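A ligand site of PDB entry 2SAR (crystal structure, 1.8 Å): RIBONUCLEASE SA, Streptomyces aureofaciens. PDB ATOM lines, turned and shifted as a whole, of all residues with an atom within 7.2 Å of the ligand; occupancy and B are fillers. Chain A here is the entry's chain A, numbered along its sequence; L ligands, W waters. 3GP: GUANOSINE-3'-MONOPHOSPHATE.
The guanidinium group (NE) of Arg 69 is in hydrogen-bond range of the side-chain hydroxyl (OH) of Tyr 86, at 3.3 Å. The guanidinium group of Arg 40 lies within hydrogen-bond range of the side-chain amide oxygen of Gln 38. The side-chain carboxylate (OE1) of Glu 54 lies within salt-bridge range of the guanidinium group (NH1) of Arg 65 (2.9 Å). The guanidinium group (NH1) of Arg 69 is in hydrogen-bond range of the backbone carbonyl oxygen (O) of Arg 65, at 3.0 Å. NH1 of Arg 65 sits at hydrogen-bond distance from OG1 of Thr 56 (2.7 Å). The side-chain carboxylate (OE1) of Glu 54 is in salt-bridge range of the guanidinium group (NE) of Arg 69, at 3.7 Å. The backbone carbonyl oxygen (O) of Val 35 lies within hydrogen-bond range of the backbone NH (N) of Glu 54, at 2.7 Å. NH2 of Arg 69 sits at hydrogen-bond distance from O of Gly 66, 2.9 Å away.
Residues that only touch the ligand: Glu 54 (2.8 Å), Phe 37 (3.4 Å), Val 35 (3.5 Å) and Val 36 (3.998 Å). Of the 20 residues printed, 13 come within 4 Å of the ligand. Along chain A the residues within 4 Å of the ligand span positions 32 to 86. The nearest printed residue that does not touch the ligand is Gly 66 (5.4 Å).
Water W1 bridges O2P of the ligand and OE1 of Gln 32. Water W4 lies within hydrogen-bond range of an oxygen (O3P) of the ligand and the guanidinium group (NH2) of Arg 69. Water W3 bridges O of Val 36 (2.5 Å) and O5' of the ligand (3.1 Å). Water W2 lies within hydrogen-bond range of OE2 of Glu 41 (3.0 Å) and N1 of the ligand (3.3 Å).
An oxygen (O3P) of the ligand lies within hydrogen-bond range of a ring nitrogen (NE2) of His 85, 2.5 Å away. A nitrogen (N1) of the ligand is in hydrogen-bond range of the side-chain carboxylate (OE1) of Glu 41 (2.6 Å). OH of Tyr 86 sits at hydrogen-bond distance from O1P of the ligand, at 2.7 Å. O6 of the ligand lies within hydrogen-bond range of N of Arg 40 (2.7 Å). The guanidinium group (NH2) of Arg 65 lies within salt-bridge range of an oxygen (O2P) of the ligand (2.8 Å). The backbone NH of Asn 39 sits at hydrogen-bond distance from an oxygen (O6) of the ligand, 2.8 Å away. The backbone NH of Gln 38 is in hydrogen-bond range of a nitrogen (N7) of the ligand (2.9 Å). An oxygen (O1P) of the ligand lies within salt-bridge range of the guanidinium group (NE) of Arg 69 (3.1 Å). The side-chain amide nitrogen (NE2) of Gln 32 lies close to an oxygen (O2P) of the ligand, at 3.1 Å.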
ATOM      1  N   GLN A  32      22.189 -18.516  10.317  1.00  0.00           N
ATOM      2  CA  GLN A  32      22.694 -18.972  11.606  1.00  0.00           C
ATOM      3  C   GLN A  32      22.767 -20.527  11.819  1.00  0.00           C
ATOM      4  O   GLN A  32      23.219 -21.068  12.867  1.00  0.00           O
ATOM      5  CB  GLN A  32      21.797 -18.709  12.881  1.00  0.00           C
ATOM      6  CG  GLN A  32      21.667 -17.316  13.405  1.00  0.00           C
ATOM      7  CD  GLN A  32      21.769 -16.831  14.840  1.00  0.00           C
ATOM      8  OE1 GLN A  32      21.660 -15.674  15.361  1.00  0.00           O
ATOM      9  NE2 GLN A  32      22.024 -17.794  15.741  1.00  0.00           N
ATOM     10  N   VAL A  35      26.189 -22.706  12.962  1.00  0.00           N
ATOM     11  CA  VAL A  35      27.208 -22.015  13.773  1.00  0.00           C
ATOM     12  C   VAL A  35      27.509 -22.970  14.970  1.00  0.00           C
ATOM     13  O   VAL A  35      26.708 -23.788  15.435  1.00  0.00           O
ATOM     14  CB  VAL A  35      26.729 -20.677  14.302  1.00  0.00           C
ATOM     15  CG1 VAL A  35      26.647 -19.709  13.142  1.00  0.00           C
ATOM     16  CG2 VAL A  35      25.395 -20.591  15.025  1.00  0.00           C
ATOM     17  N   VAL A  36      28.673 -22.630  15.515  1.00  0.00           N
ATOM     18  CA  VAL A  36      29.192 -23.323  16.736  1.00  0.00           C
ATOM     19  C   VAL A  36      28.314 -23.012  17.908  1.00  0.00           C
ATOM     20  O   VAL A  36      27.865 -21.894  18.162  1.00  0.00           O
ATOM     21  CB  VAL A  36      30.684 -22.947  17.094  1.00  0.00           C
ATOM     22  CG1 VAL A  36      31.258 -23.675  18.296  1.00  0.00           C
ATOM     23  CG2 VAL A  36      31.517 -23.391  15.927  1.00  0.00           C
ATOM     24  N   PHE A  37      28.088 -24.039  18.724  1.00  0.00           N
ATOM     25  CA  PHE A  37      27.407 -23.959  19.995  1.00  0.00           C
ATOM     26  C   PHE A  37      28.595 -24.045  20.970  1.00  0.00           C
ATOM     27  O   PHE A  37      29.277 -25.069  20.874  1.00  0.00           O
ATOM     28  CB  PHE A  37      26.379 -25.087  20.205  1.00  0.00           C
ATOM     29  CG  PHE A  37      25.722 -24.999  21.553  1.00  0.00           C
ATOM     30  CD1 PHE A  37      24.813 -23.985  21.847  1.00  0.00           C
ATOM     31  CD2 PHE A  37      26.038 -25.980  22.518  1.00  0.00           C
ATOM     32  CE1 PHE A  37      24.228 -23.911  23.123  1.00  0.00           C
ATOM     33  CE2 PHE A  37      25.428 -25.932  23.754  1.00  0.00           C
ATOM     34  CZ  PHE A  37      24.540 -24.883  24.052  1.00  0.00           C
ATOM     35  N   GLN A  38      28.712 -23.074  21.856  1.00  0.00           N
ATOM     36  CA  GLN A  38      29.852 -23.111  22.793  1.00  0.00           C
ATOM     37  C   GLN A  38      29.785 -24.015  24.015  1.00  0.00           C
ATOM     38  O   GLN A  38      30.900 -24.316  24.533  1.00  0.00           O
ATOM     39  CB  GLN A  38      30.022 -21.693  23.366  1.00  0.00           C
ATOM     40  CG  GLN A  38      30.645 -20.801  22.317  1.00  0.00           C
ATOM     41  CD  GLN A  38      30.864 -19.501  23.118  1.00  0.00           C
ATOM     42  OE1 GLN A  38      31.502 -19.476  24.209  1.00  0.00           O
ATOM     43  NE2 GLN A  38      30.290 -18.431  22.620  1.00  0.00           N
ATOM     44  N   ASN A  39      28.592 -24.403  24.397  1.00  0.00           N
ATOM     45  CA  ASN A  39      28.396 -25.269  25.583  1.00  0.00           C
ATOM     46  C   ASN A  39      28.972 -24.515  26.817  1.00  0.00           C
ATOM     47  O   ASN A  39      29.581 -25.121  27.725  1.00  0.00           O
ATOM     48  CB  ASN A  39      29.103 -26.636  25.393  1.00  0.00           C
ATOM     49  CG  ASN A  39      28.711 -27.614  26.493  1.00  0.00           C
ATOM     50  OD1 ASN A  39      27.604 -27.496  27.010  1.00  0.00           O
ATOM     51  ND2 ASN A  39      29.621 -28.511  26.921  1.00  0.00           N
ATOM     52  N   ARG A  40      28.812 -23.230  26.833  1.00  0.00           N
ATOM     53  CA  ARG A  40      29.347 -22.335  27.893  1.00  0.00           C
ATOM     54  C   ARG A  40      28.892 -22.657  29.311  1.00  0.00           C
ATOM     55  O   ARG A  40      29.715 -22.534  30.270  1.00  0.00           O
ATOM     56  CB  ARG A  40      29.111 -20.891  27.408  1.00  0.00           C
ATOM     57  CG  ARG A  40      29.429 -19.816  28.430  1.00  0.00           C
ATOM     58  CD  ARG A  40      29.594 -18.459  27.780  1.00  0.00           C
ATOM     59  NE  ARG A  40      30.970 -18.124  27.505  1.00  0.00           N
ATOM     60  CZ  ARG A  40      32.185 -17.628  27.596  1.00  0.00           C
ATOM     61  NH1 ARG A  40      32.916 -17.369  28.696  1.00  0.00           N
ATOM     62  NH2 ARG A  40      32.773 -17.329  26.397  1.00  0.00           N
ATOM     63  N   GLU A  41      27.654 -23.128  29.403  1.00  0.00           N
ATOM     64  CA  GLU A  41      27.113 -23.501  30.707  1.00  0.00           C
ATOM     65  C   GLU A  41      27.440 -24.906  31.187  1.00  0.00           C
ATOM     66  O   GLU A  41      26.986 -25.331  32.294  1.00  0.00           O
ATOM     67  CB  GLU A  41      25.579 -23.320  30.732  1.00  0.00           C
ATOM     68  CG  GLU A  41      25.179 -21.858  30.561  1.00  0.00           C
ATOM     69  CD  GLU A  41      25.322 -21.460  29.093  1.00  0.00           C
ATOM     70  OE1 GLU A  41      25.103 -22.173  28.097  1.00  0.00           O
ATOM     71  OE2 GLU A  41      25.749 -20.271  29.075  1.00  0.00           O
ATOM     72  N   SER A  42      28.178 -25.616  30.383  1.00  0.00           N
ATOM     73  CA  SER A  42      28.565 -27.013  30.613  1.00  0.00           C
ATOM     74  C   SER A  42      27.373 -27.958  30.805  1.00  0.00           C
ATOM     75  O   SER A  42      27.529 -28.925  31.573  1.00  0.00           O
ATOM     76  CB  SER A  42      29.693 -26.997  31.730  1.00  0.00           C
ATOM     77  OG  SER A  42      30.330 -28.367  31.562  1.00  0.00           O
ATOM     78  N   GLU A  54      24.868 -25.606  16.156  1.00  0.00           N
ATOM     79  CA  GLU A  54      23.411 -25.455  16.437  1.00  0.00           C
ATOM     80  C   GLU A  54      22.590 -25.276  15.114  1.00  0.00           C
ATOM     81  O   GLU A  54      23.053 -24.614  14.165  1.00  0.00           O
ATOM     82  CB  GLU A  54      23.259 -24.262  17.290  1.00  0.00           C
ATOM     83  CG  GLU A  54      22.362 -23.192  17.785  1.00  0.00           C
ATOM     84  CD  GLU A  54      21.785 -22.337  16.665  1.00  0.00           C
ATOM     85  OE1 GLU A  54      20.756 -22.683  16.047  1.00  0.00           O
ATOM     86  OE2 GLU A  54      22.520 -21.374  16.446  1.00  0.00           O
ATOM     87  N   THR A  56      18.335 -24.605  13.802  1.00  0.00           N
ATOM     88  CA  THR A  56      16.979 -24.368  14.280  1.00  0.00           C
ATOM     89  C   THR A  56      16.008 -25.518  14.008  1.00  0.00           C
ATOM     90  O   THR A  56      16.108 -26.136  12.948  1.00  0.00           O
ATOM     91  CB  THR A  56      16.357 -23.158  13.431  1.00  0.00           C
ATOM     92  OG1 THR A  56      17.452 -22.243  13.322  1.00  0.00           O
ATOM     93  CG2 THR A  56      15.023 -22.746  14.051  1.00  0.00           C
ATOM     94  N   ARG A  65      12.914 -17.288  15.509  1.00  0.00           N
ATOM     95  CA  ARG A  65      13.394 -18.688  15.383  1.00  0.00           C
ATOM     96  C   ARG A  65      12.917 -19.574  16.548  1.00  0.00           C
ATOM     97  O   ARG A  65      13.114 -20.798  16.655  1.00  0.00           O
ATOM     98  CB  ARG A  65      14.896 -18.647  15.284  1.00  0.00           C
ATOM     99  CG  ARG A  65      15.649 -18.275  14.075  1.00  0.00           C
ATOM    100  CD  ARG A  65      17.040 -18.818  13.940  1.00  0.00           C
ATOM    101  NE  ARG A  65      17.969 -18.502  14.995  1.00  0.00           N
ATOM    102  CZ  ARG A  65      18.636 -19.529  15.545  1.00  0.00           C
ATOM    103  NH1 ARG A  65      18.687 -20.824  15.291  1.00  0.00           N
ATOM    104  NH2 ARG A  65      19.331 -18.999  16.503  1.00  0.00           N
ATOM    105  N   GLY A  66      12.247 -18.993  17.545  1.00  0.00           N
ATOM    106  CA  GLY A  66      11.669 -19.555  18.744  1.00  0.00           C
ATOM    107  C   GLY A  66      12.800 -20.210  19.609  1.00  0.00           C
ATOM    108  O   GLY A  66      13.961 -19.775  19.621  1.00  0.00           O
ATOM    109  N   ARG A  68      13.270 -23.981  19.875  1.00  0.00           N
ATOM    110  CA  ARG A  68      13.679 -25.334  19.591  1.00  0.00           C
ATOM    111  C   ARG A  68      14.917 -25.306  18.754  1.00  0.00           C
ATOM    112  O   ARG A  68      15.069 -24.544  17.789  1.00  0.00           O
ATOM    113  CB  ARG A  68      12.520 -26.087  18.922  1.00  0.00           C
ATOM    114  CG  ARG A  68      11.252 -25.887  19.756  1.00  0.00           C
ATOM    115  CD  ARG A  68      10.176 -26.680  19.011  1.00  0.00           C
ATOM    116  NE  ARG A  68       9.000 -26.326  19.803  1.00  0.00           N
ATOM    117  CZ  ARG A  68       7.745 -26.734  19.549  1.00  0.00           C
ATOM    118  NH1 ARG A  68       7.415 -27.420  18.482  1.00  0.00           N
ATOM    119  NH2 ARG A  68       6.809 -26.424  20.438  1.00  0.00           N
ATOM    120  N   ARG A  69      15.824 -26.251  19.114  1.00  0.00           N
ATOM    121  CA  ARG A  69      17.104 -26.380  18.402  1.00  0.00           C
ATOM    122  C   ARG A  69      17.562 -27.828  18.493  1.00  0.00           C
ATOM    123  O   ARG A  69      17.176 -28.624  19.373  1.00  0.00           O
ATOM    124  CB  ARG A  69      18.301 -25.589  19.060  1.00  0.00           C
ATOM    125  CG  ARG A  69      17.927 -24.147  19.408  1.00  0.00           C
ATOM    126  CD  ARG A  69      18.071 -23.356  18.122  1.00  0.00           C
ATOM    127  NE  ARG A  69      17.889 -21.894  18.322  1.00  0.00           N
ATOM    128  CZ  ARG A  69      16.687 -21.261  18.361  1.00  0.00           C
ATOM    129  NH1 ARG A  69      15.522 -21.862  18.164  1.00  0.00           N
ATOM    130  NH2 ARG A  69      16.653 -19.958  18.657  1.00  0.00           N
ATOM    131  N   ILE A  71      21.218 -29.659  18.518  1.00  0.00           N
ATOM    132  CA  ILE A  71      22.677 -29.541  18.733  1.00  0.00           C
ATOM    133  C   ILE A  71      23.373 -30.791  18.222  1.00  0.00           C
ATOM    134  O   ILE A  71      23.156 -31.899  18.768  1.00  0.00           O
ATOM    135  CB  ILE A  71      23.170 -29.220  20.202  1.00  0.00           C
ATOM    136  CG1 ILE A  71      22.380 -28.051  20.836  1.00  0.00           C
ATOM    137  CG2 ILE A  71      24.746 -29.024  20.231  1.00  0.00           C
ATOM    138  CD1 ILE A  71      22.483 -26.701  20.074  1.00  0.00           C
ATOM    139  N   HIS A  85      15.384 -23.322  24.688  1.00  0.00           N
ATOM    140  CA  HIS A  85      16.477 -22.477  24.251  1.00  0.00           C
ATOM    141  C   HIS A  85      17.748 -22.762  25.049  1.00  0.00           C
ATOM    142  O   HIS A  85      18.237 -21.840  25.725  1.00  0.00           O
ATOM    143  CB  HIS A  85      15.967 -21.000  24.372  1.00  0.00           C
ATOM    144  CG  HIS A  85      16.963 -20.081  23.740  1.00  0.00           C
ATOM    145  ND1 HIS A  85      18.016 -19.479  24.422  1.00  0.00           N
ATOM    146  CD2 HIS A  85      17.047 -19.633  22.454  1.00  0.00           C
ATOM    147  CE1 HIS A  85      18.708 -18.717  23.567  1.00  0.00           C
ATOM    148  NE2 HIS A  85      18.121 -18.770  22.391  1.00  0.00           N
ATOM    149  N   TYR A  86      18.218 -24.016  24.946  1.00  0.00           N
ATOM    150  CA  TYR A  86      19.458 -24.499  25.561  1.00  0.00           C
ATOM    151  C   TYR A  86      19.367 -24.688  27.068  1.00  0.00           C
ATOM    152  O   TYR A  86      20.491 -24.852  27.590  1.00  0.00           O
ATOM    153  CB  TYR A  86      20.635 -23.535  25.276  1.00  0.00           C
ATOM    154  CG  TYR A  86      20.647 -23.004  23.872  1.00  0.00           C
ATOM    155  CD1 TYR A  86      20.784 -23.969  22.845  1.00  0.00           C
ATOM    156  CD2 TYR A  86      20.572 -21.632  23.538  1.00  0.00           C
ATOM    157  CE1 TYR A  86      20.867 -23.546  21.512  1.00  0.00           C
ATOM    158  CE2 TYR A  86      20.586 -21.246  22.202  1.00  0.00           C
ATOM    159  CZ  TYR A  86      20.697 -22.200  21.189  1.00  0.00           C
ATOM    160  OH  TYR A  86      20.774 -21.925  19.861  1.00  0.00           O
ATOM    161  N   ALA A  87      18.263 -24.652  27.770  1.00  0.00           N
ATOM    162  CA  ALA A  87      18.158 -24.917  29.197  1.00  0.00           C
ATOM    163  C   ALA A  87      18.340 -26.445  29.470  1.00  0.00           C
ATOM    164  O   ALA A  87      19.107 -26.865  30.381  1.00  0.00           O
ATOM    165  CB  ALA A  87      16.853 -24.359  29.763  1.00  0.00           C
ATOM    166  N   PHE A  89      18.419 -30.669  27.461  1.00  0.00           N
ATOM    167  CA  PHE A  89      18.773 -31.342  26.187  1.00  0.00           C
ATOM    168  C   PHE A  89      18.409 -32.791  26.366  1.00  0.00           C
ATOM    169  O   PHE A  89      18.551 -33.266  27.500  1.00  0.00           O
ATOM    170  CB  PHE A  89      20.256 -31.315  25.835  1.00  0.00           C
ATOM    171  CG  PHE A  89      20.727 -29.885  25.690  1.00  0.00           C
ATOM    172  CD1 PHE A  89      21.061 -29.110  26.807  1.00  0.00           C
ATOM    173  CD2 PHE A  89      20.820 -29.300  24.408  1.00  0.00           C
ATOM    174  CE1 PHE A  89      21.473 -27.806  26.681  1.00  0.00           C
ATOM    175  CE2 PHE A  89      21.293 -27.979  24.244  1.00  0.00           C
ATOM    176  CZ  PHE A  89      21.656 -27.246  25.392  1.00  0.00           C
HETATM  177  P   3GP L   1      19.971 -18.074  19.495  1.00  0.00           P
HETATM  178  O1P 3GP L   1      19.693 -19.587  19.209  1.00  0.00           O
HETATM  179  O2P 3GP L   1      20.353 -17.162  18.330  1.00  0.00           O
HETATM  180  O3P 3GP L   1      18.857 -17.505  20.318  1.00  0.00           O
HETATM  181  O5' 3GP L   1      25.026 -18.714  18.262  1.00  0.00           O
HETATM  182  C5' 3GP L   1      23.718 -19.278  17.844  1.00  0.00           C
HETATM  183  C4' 3GP L   1      22.807 -19.260  19.089  1.00  0.00           C
HETATM  184  O4' 3GP L   1      23.454 -20.134  20.067  1.00  0.00           O
HETATM  185  C3' 3GP L   1      22.545 -17.948  19.814  1.00  0.00           C
HETATM  186  O3' 3GP L   1      21.295 -17.954  20.472  1.00  0.00           O
HETATM  187  C2' 3GP L   1      23.603 -17.840  20.926  1.00  0.00           C
HETATM  188  O2' 3GP L   1      23.068 -17.201  22.093  1.00  0.00           O
HETATM  189  C1' 3GP L   1      23.648 -19.326  21.298  1.00  0.00           C
HETATM  190  N9  3GP L   1      24.823 -19.954  21.933  1.00  0.00           N
HETATM  191  C8  3GP L   1      26.034 -20.387  21.381  1.00  0.00           C
HETATM  192  N7  3GP L   1      26.749 -21.014  22.281  1.00  0.00           N
HETATM  193  C5  3GP L   1      25.949 -20.949  23.463  1.00  0.00           C
HETATM  194  C6  3GP L   1      26.085 -21.491  24.794  1.00  0.00           C
HETATM  195  O6  3GP L   1      27.097 -22.113  25.134  1.00  0.00           O
HETATM  196  N1  3GP L   1      24.989 -21.219  25.640  1.00  0.00           N
HETATM  197  C2  3GP L   1      23.806 -20.548  25.335  1.00  0.00           C
HETATM  198  N2  3GP L   1      22.886 -20.443  26.304  1.00  0.00           N
HETATM  199  N3  3GP L   1      23.682 -20.087  24.110  1.00  0.00           N
HETATM  200  C4  3GP L   1      24.716 -20.303  23.268  1.00  0.00           C
HETATM  201  O   HOH W   1      21.515 -14.696  18.352  1.00  0.00           O
HETATM  202  O   HOH W   2      25.374 -18.222  26.970  1.00  0.00           O
HETATM  203  O   HOH W   3      27.991 -19.400  17.864  1.00  0.00           O
HETATM  204  O   HOH W   4      16.082 -16.918  19.216  1.00  0.00           O
